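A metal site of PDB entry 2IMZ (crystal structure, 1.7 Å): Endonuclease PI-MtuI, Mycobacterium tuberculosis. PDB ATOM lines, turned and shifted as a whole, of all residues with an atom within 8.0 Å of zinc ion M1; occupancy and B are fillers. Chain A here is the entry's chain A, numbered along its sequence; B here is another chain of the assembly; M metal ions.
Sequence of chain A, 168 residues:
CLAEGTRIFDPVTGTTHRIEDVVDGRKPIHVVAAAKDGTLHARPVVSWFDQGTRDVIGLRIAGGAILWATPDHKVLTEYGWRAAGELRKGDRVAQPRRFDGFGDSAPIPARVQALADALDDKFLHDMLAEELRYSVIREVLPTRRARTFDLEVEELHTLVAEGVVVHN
Within 4 Å of zinc ion M1: Glu 152, His 157 of chain A, SNN 168 of chain A and His 167 of chain B.
The side-chain carboxylate (OE2) of Glu 152 lies within salt-bridge range of the side-chain amino group (NZ) of Lys 74 of chain B (2.5 Å).
The backbone carbonyl oxygen of Ser 47 is in hydrogen-bond range of the backbone NH of Glu 152, at 3.0 Å.
N of Val 46 is in hydrogen-bond range of O of Glu 152.
The backbone NH (N) of His 167 of chain B sits at hydrogen-bond distance from the backbone carbonyl oxygen (O) of Lys 74 of chain B (2.8 Å).
O5 of SNN 168 of chain A sits at hydrogen-bond distance from the backbone NH of Val 153 (2.6 Å).
Zinc ion M1 is bound by a ring nitrogen (ND1) of His 157 of chain A (2.0 Å), a ring nitrogen (NE2) of His 167 of chain B (2.0 Å), N1 of SNN 168 of chain A (2.1 Å) and the side-chain carboxylate (OE1) of Glu 152 (2.2 Å).
Zinc ion M1 has four donor atoms within binding distance.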
ATOM      1  N   VAL A  46      29.632 -12.676  -2.385  1.00  0.00           N
ATOM      2  CA  VAL A  46      30.163 -11.516  -1.669  1.00  0.00           C
ATOM      3  C   VAL A  46      31.641 -11.610  -1.325  1.00  0.00           C
ATOM      4  O   VAL A  46      32.259 -10.609  -0.926  1.00  0.00           O
ATOM      5  CB  VAL A  46      29.351 -11.245  -0.393  1.00  0.00           C
ATOM      6  CG1 VAL A  46      27.934 -10.823  -0.756  1.00  0.00           C
ATOM      7  CG2 VAL A  46      29.309 -12.490   0.478  1.00  0.00           C
ATOM      8  N   SER A  47      32.217 -12.800  -1.471  1.00  0.00           N
ATOM      9  CA  SER A  47      33.648 -13.011  -1.192  1.00  0.00           C
ATOM     10  C   SER A  47      34.207 -13.991  -2.209  1.00  0.00           C
ATOM     11  O   SER A  47      33.502 -14.886  -2.680  1.00  0.00           O
ATOM     12  CB  SER A  47      33.856 -13.567   0.218  1.00  0.00           C
ATOM     13  OG  SER A  47      33.367 -12.675   1.205  1.00  0.00           O
ATOM     14  N   PHE A  49      37.756 -16.472  -3.113  1.00  0.00           N
ATOM     15  CA  PHE A  49      39.000 -17.046  -2.593  1.00  0.00           C
ATOM     16  C   PHE A  49      39.767 -17.902  -3.594  1.00  0.00           C
ATOM     17  O   PHE A  49      39.212 -18.815  -4.211  1.00  0.00           O
ATOM     18  CB  PHE A  49      38.719 -17.877  -1.343  1.00  0.00           C
ATOM     19  CG  PHE A  49      37.899 -17.158  -0.301  1.00  0.00           C
ATOM     20  CD1 PHE A  49      36.508 -17.145  -0.378  1.00  0.00           C
ATOM     21  CD2 PHE A  49      38.520 -16.456   0.726  1.00  0.00           C
ATOM     22  CE1 PHE A  49      35.746 -16.453   0.558  1.00  0.00           C
ATOM     23  CE2 PHE A  49      37.768 -15.756   1.674  1.00  0.00           C
ATOM     24  CZ  PHE A  49      36.373 -15.763   1.589  1.00  0.00           C
ATOM     25  N   ASP A 150      37.067 -20.915  -3.980  1.00  0.00           N
ATOM     26  CA  ASP A 150      35.912 -20.944  -3.103  1.00  0.00           C
ATOM     27  C   ASP A 150      35.171 -19.617  -3.234  1.00  0.00           C
ATOM     28  O   ASP A 150      35.753 -18.615  -3.633  1.00  0.00           O
ATOM     29  CB  ASP A 150      36.388 -21.152  -1.657  1.00  0.00           C
ATOM     30  CG  ASP A 150      35.312 -21.744  -0.769  1.00  0.00           C
ATOM     31  OD1 ASP A 150      34.675 -22.739  -1.174  1.00  0.00           O
ATOM     32  OD2 ASP A 150      35.124 -21.223   0.363  1.00  0.00           O
ATOM     33  N   LEU A 151      33.875 -19.624  -2.914  1.00  0.00           N
ATOM     34  CA  LEU A 151      33.050 -18.424  -3.005  1.00  0.00           C
ATOM     35  C   LEU A 151      32.153 -18.309  -1.778  1.00  0.00           C
ATOM     36  O   LEU A 151      31.729 -19.319  -1.230  1.00  0.00           O
ATOM     37  CB  LEU A 151      32.158 -18.476  -4.248  1.00  0.00           C
ATOM     38  CG  LEU A 151      32.813 -18.578  -5.627  1.00  0.00           C
ATOM     39  CD1 LEU A 151      31.739 -18.862  -6.691  1.00  0.00           C
ATOM     40  CD2 LEU A 151      33.543 -17.280  -5.941  1.00  0.00           C
ATOM     41  N   GLU A 152      31.873 -17.077  -1.358  1.00  0.00           N
ATOM     42  CA  GLU A 152      30.966 -16.862  -0.245  1.00  0.00           C
ATOM     43  C   GLU A 152      29.688 -16.304  -0.845  1.00  0.00           C
ATOM     44  O   GLU A 152      29.720 -15.331  -1.599  1.00  0.00           O
ATOM     45  CB  GLU A 152      31.515 -15.862   0.775  1.00  0.00           C
ATOM     46  CG  GLU A 152      32.387 -16.492   1.854  1.00  0.00           C
ATOM     47  CD  GLU A 152      31.709 -17.647   2.578  1.00  0.00           C
ATOM     48  OE1 GLU A 152      30.621 -17.456   3.184  1.00  0.00           O
ATOM     49  OE2 GLU A 152      32.273 -18.750   2.550  1.00  0.00           O
ATOM     50  N   VAL A 153      28.579 -16.940  -0.505  1.00  0.00           N
ATOM     51  CA  VAL A 153      27.250 -16.567  -0.982  1.00  0.00           C
ATOM     52  C   VAL A 153      26.472 -15.948   0.172  1.00  0.00           C
ATOM     53  O   VAL A 153      26.296 -16.577   1.217  1.00  0.00           O
ATOM     54  CB  VAL A 153      26.493 -17.808  -1.515  1.00  0.00           C
ATOM     55  CG1 VAL A 153      25.092 -17.420  -1.962  1.00  0.00           C
ATOM     56  CG2 VAL A 153      27.261 -18.424  -2.672  1.00  0.00           C
ATOM     57  N   GLU A 154      26.018 -14.719  -0.023  1.00  0.00           N
ATOM     58  CA  GLU A 154      25.272 -14.025   1.001  1.00  0.00           C
ATOM     59  C   GLU A 154      24.122 -14.825   1.621  1.00  0.00           C
ATOM     60  O   GLU A 154      23.370 -15.502   0.921  1.00  0.00           O
ATOM     61  CB  GLU A 154      24.721 -12.710   0.441  1.00  0.00           C
ATOM     62  CG  GLU A 154      23.779 -11.991   1.386  1.00  0.00           C
ATOM     63  CD  GLU A 154      23.101 -10.811   0.719  1.00  0.00           C
ATOM     64  OE1 GLU A 154      23.794  -9.814   0.446  1.00  0.00           O
ATOM     65  OE2 GLU A 154      21.882 -10.900   0.454  1.00  0.00           O
ATOM     66  N   GLU A 155      24.029 -14.731   2.945  1.00  0.00           N
ATOM     67  CA  GLU A 155      22.988 -15.362   3.755  1.00  0.00           C
ATOM     68  C   GLU A 155      22.870 -16.889   3.822  1.00  0.00           C
ATOM     69  O   GLU A 155      22.950 -17.461   4.906  1.00  0.00           O
ATOM     70  CB  GLU A 155      21.620 -14.769   3.366  1.00  0.00           C
ATOM     71  CG  GLU A 155      20.453 -15.348   4.175  1.00  0.00           C
ATOM     72  CD  GLU A 155      19.091 -14.813   3.745  1.00  0.00           C
ATOM     73  OE1 GLU A 155      18.841 -14.703   2.524  1.00  0.00           O
ATOM     74  OE2 GLU A 155      18.250 -14.522   4.622  1.00  0.00           O
ATOM     75  N   LEU A 156      22.676 -17.529   2.680  1.00  0.00           N
ATOM     76  CA  LEU A 156      22.464 -18.980   2.668  1.00  0.00           C
ATOM     77  C   LEU A 156      23.685 -19.890   2.713  1.00  0.00           C
ATOM     78  O   LEU A 156      23.552 -21.064   3.053  1.00  0.00           O
ATOM     79  CB  LEU A 156      21.571 -19.332   1.486  1.00  0.00           C
ATOM     80  CG  LEU A 156      20.238 -18.578   1.542  1.00  0.00           C
ATOM     81  CD1 LEU A 156      19.366 -18.949   0.348  1.00  0.00           C
ATOM     82  CD2 LEU A 156      19.521 -18.916   2.842  1.00  0.00           C
ATOM     83  N   HIS A 157      24.856 -19.369   2.377  1.00  0.00           N
ATOM     84  CA  HIS A 157      26.083 -20.163   2.446  1.00  0.00           C
ATOM     85  C   HIS A 157      26.125 -21.444   1.634  1.00  0.00           C
ATOM     86  O   HIS A 157      26.801 -22.404   2.001  1.00  0.00           O
ATOM     87  CB  HIS A 157      26.392 -20.474   3.906  1.00  0.00           C
ATOM     88  CG  HIS A 157      26.810 -19.281   4.700  1.00  0.00           C
ATOM     89  ND1 HIS A 157      28.081 -18.769   4.656  1.00  0.00           N
ATOM     90  CD2 HIS A 157      26.102 -18.457   5.524  1.00  0.00           C
ATOM     91  CE1 HIS A 157      28.154 -17.679   5.406  1.00  0.00           C
ATOM     92  NE2 HIS A 157      26.959 -17.480   5.939  1.00  0.00           N
ATOM     93  N   THR A 158      25.393 -21.474   0.525  1.00  0.00           N
ATOM     94  CA  THR A 158      25.383 -22.637  -0.352  1.00  0.00           C
ATOM     95  C   THR A 158      25.308 -22.149  -1.799  1.00  0.00           C
ATOM     96  O   THR A 158      25.004 -20.984  -2.047  1.00  0.00           O
ATOM     97  CB  THR A 158      24.165 -23.570  -0.086  1.00  0.00           C
ATOM     98  OG1 THR A 158      22.953 -22.882  -0.364  1.00  0.00           O
ATOM     99  CG2 THR A 158      24.165 -24.056   1.361  1.00  0.00           C
ATOM    100  N   LEU A 159      25.602 -23.027  -2.747  1.00  0.00           N
ATOM    101  CA  LEU A 159      25.546 -22.657  -4.158  1.00  0.00           C
ATOM    102  C   LEU A 159      25.565 -23.893  -5.026  1.00  0.00           C
ATOM    103  O   LEU A 159      25.989 -24.967  -4.593  1.00  0.00           O
ATOM    104  CB  LEU A 159      26.730 -21.767  -4.563  1.00  0.00           C
ATOM    105  CG  LEU A 159      28.088 -22.460  -4.675  1.00  0.00           C
ATOM    106  CD1 LEU A 159      28.997 -21.693  -5.628  1.00  0.00           C
ATOM    107  CD2 LEU A 159      28.701 -22.581  -3.301  1.00  0.00           C
ATOM    108  N   HIS A 167      28.463 -26.933  -0.406  1.00  0.00           N
ATOM    109  CA  HIS A 167      28.630 -26.052   0.740  1.00  0.00           C
ATOM    110  C   HIS A 167      29.477 -24.834   0.430  1.00  0.00           C
ATOM    111  O   HIS A 167      30.526 -24.941  -0.211  1.00  0.00           O
ATOM    112  CB  HIS A 167      29.253 -26.859   1.886  1.00  0.00           C
ATOM    113  CG  HIS A 167      29.298 -26.136   3.194  1.00  0.00           C
ATOM    114  ND1 HIS A 167      30.326 -25.294   3.532  1.00  0.00           N
ATOM    115  CD2 HIS A 167      28.453 -26.147   4.247  1.00  0.00           C
ATOM    116  CE1 HIS A 167      30.117 -24.823   4.750  1.00  0.00           C
ATOM    117  NE2 HIS A 167      28.981 -25.325   5.198  1.00  0.00           N
ATOM    118  N1  SNN A 168      29.746 -20.692   2.284  1.00  0.00           N
ATOM    119  C   SNN A 168      30.180 -21.946   2.214  1.00  0.00           C
ATOM    120  CA  SNN A 168      29.952 -22.469   0.812  1.00  0.00           C
ATOM    121  N   SNN A 168      29.067 -23.633   0.851  1.00  0.00           N
ATOM    122  C4  SNN A 168      29.314 -21.277   0.070  1.00  0.00           C
ATOM    123  C5  SNN A 168      29.244 -20.209   1.141  1.00  0.00           C
ATOM    124  O   SNN A 168      30.668 -22.580   3.126  1.00  0.00           O
ATOM    125  O5  SNN A 168      28.808 -19.088   0.991  1.00  0.00           O
ATOM    126  N   LYS B  74      37.453 -19.248   7.500  1.00  0.00           N
ATOM    127  CA  LYS B  74      36.864 -17.916   7.378  1.00  0.00           C
ATOM    128  C   LYS B  74      36.411 -17.315   8.697  1.00  0.00           C
ATOM    129  O   LYS B  74      35.791 -17.975   9.532  1.00  0.00           O
ATOM    130  CB  LYS B  74      35.713 -17.960   6.368  1.00  0.00           C
ATOM    131  CG  LYS B  74      36.221 -18.134   4.940  1.00  0.00           C
ATOM    132  CD  LYS B  74      35.125 -18.510   3.959  1.00  0.00           C
ATOM    133  CE  LYS B  74      34.685 -19.952   4.187  1.00  0.00           C
ATOM    134  NZ  LYS B  74      33.933 -20.507   3.025  1.00  0.00           N
ATOM    135  N   TRP B  81      33.575 -11.748   5.211  1.00  0.00           N
ATOM    136  CA  TRP B  81      34.305 -12.980   5.429  1.00  0.00           C
ATOM    137  C   TRP B  81      35.688 -12.942   4.802  1.00  0.00           C
ATOM    138  O   TRP B  81      35.843 -12.644   3.618  1.00  0.00           O
ATOM    139  CB  TRP B  81      33.527 -14.174   4.872  1.00  0.00           C
ATOM    140  CG  TRP B  81      32.221 -14.390   5.571  1.00  0.00           C
ATOM    141  CD1 TRP B  81      30.973 -14.041   5.120  1.00  0.00           C
ATOM    142  CD2 TRP B  81      32.029 -14.940   6.872  1.00  0.00           C
ATOM    143  NE1 TRP B  81      30.030 -14.355   6.060  1.00  0.00           N
ATOM    144  CE2 TRP B  81      30.647 -14.912   7.152  1.00  0.00           C
ATOM    145  CE3 TRP B  81      32.901 -15.473   7.840  1.00  0.00           C
ATOM    146  CZ2 TRP B  81      30.108 -15.379   8.354  1.00  0.00           C
ATOM    147  CZ3 TRP B  81      32.362 -15.940   9.042  1.00  0.00           C
ATOM    148  CH2 TRP B  81      30.988 -15.885   9.288  1.00  0.00           C
ATOM    149  N   LEU B 156      22.220 -21.154   9.835  1.00  0.00           N
ATOM    150  CA  LEU B 156      23.098 -19.990   9.752  1.00  0.00           C
ATOM    151  C   LEU B 156      24.552 -20.219   9.368  1.00  0.00           C
ATOM    152  O   LEU B 156      25.225 -19.281   8.931  1.00  0.00           O
ATOM    153  CB  LEU B 156      23.005 -19.212  11.065  1.00  0.00           C
ATOM    154  CG  LEU B 156      21.582 -18.774  11.412  1.00  0.00           C
ATOM    155  CD1 LEU B 156      21.602 -17.971  12.700  1.00  0.00           C
ATOM    156  CD2 LEU B 156      20.992 -17.945  10.283  1.00  0.00           C
ATOM    157  N   HIS B 157      25.044 -21.443   9.519  1.00  0.00           N
ATOM    158  CA  HIS B 157      26.407 -21.778   9.149  1.00  0.00           C
ATOM    159  C   HIS B 157      27.508 -20.946   9.792  1.00  0.00           C
ATOM    160  O   HIS B 157      28.574 -20.760   9.200  1.00  0.00           O
ATOM    161  CB  HIS B 157      26.547 -21.714   7.622  1.00  0.00           C
ATOM    162  CG  HIS B 157      25.802 -22.795   6.898  1.00  0.00           C
ATOM    163  ND1 HIS B 157      26.329 -24.050   6.675  1.00  0.00           N
ATOM    164  CD2 HIS B 157      24.540 -22.816   6.389  1.00  0.00           C
ATOM    165  CE1 HIS B 157      25.429 -24.797   6.062  1.00  0.00           C
ATOM    166  NE2 HIS B 157      24.339 -24.078   5.875  1.00  0.00           N
ATOM    167  N   THR B 158      27.260 -20.442  10.994  1.00  0.00           N
ATOM    168  CA  THR B 158      28.252 -19.643  11.707  1.00  0.00           C
ATOM    169  C   THR B 158      28.182 -19.986  13.195  1.00  0.00           C
ATOM    170  O   THR B 158      27.226 -20.621  13.640  1.00  0.00           O
ATOM    171  CB  THR B 158      27.996 -18.126  11.570  1.00  0.00           C
ATOM    172  OG1 THR B 158      26.724 -17.802  12.156  1.00  0.00           O
ATOM    173  CG2 THR B 158      27.992 -17.715  10.103  1.00  0.00           C
ATOM    174  N   HIS B 167      33.286 -18.806  10.596  1.00  0.00           N
ATOM    175  CA  HIS B 167      32.509 -19.498   9.587  1.00  0.00           C
ATOM    176  C   HIS B 167      32.346 -20.978   9.939  1.00  0.00           C
ATOM    177  O   HIS B 167      33.257 -21.587  10.511  1.00  0.00           O
ATOM    178  CB  HIS B 167      33.195 -19.355   8.238  1.00  0.00           C
ATOM    179  CG  HIS B 167      32.333 -19.757   7.084  1.00  0.00           C
ATOM    180  ND1 HIS B 167      32.141 -21.073   6.728  1.00  0.00           N
ATOM    181  CD2 HIS B 167      31.595 -19.016   6.233  1.00  0.00           C
ATOM    182  CE1 HIS B 167      31.309 -21.127   5.702  1.00  0.00           C
ATOM    183  NE2 HIS B 167      30.964 -19.891   5.379  1.00  0.00           N
ATOM    184  N1  SNN B 168      29.477 -24.154   8.401  1.00  0.00           N
ATOM    185  C   SNN B 168      30.688 -23.603   8.344  1.00  0.00           C
ATOM    186  CA  SNN B 168      31.035 -23.048   9.710  1.00  0.00           C
ATOM    187  N   SNN B 168      31.207 -21.582   9.625  1.00  0.00           N
ATOM    188  C4  SNN B 168      29.820 -23.395  10.582  1.00  0.00           C
ATOM    189  C5  SNN B 168      28.896 -24.101   9.609  1.00  0.00           C
ATOM    190  O   SNN B 168      31.383 -23.549   7.359  1.00  0.00           O
ATOM    191  O5  SNN B 168      27.804 -24.536   9.879  1.00  0.00           O
HETATM  192 ZN    ZN M   1      29.776 -19.363   3.863  1.00  0.00          ZN
HETATM  193 ZN    ZN M   2      28.130 -24.946   7.002  1.00  0.00          ZN
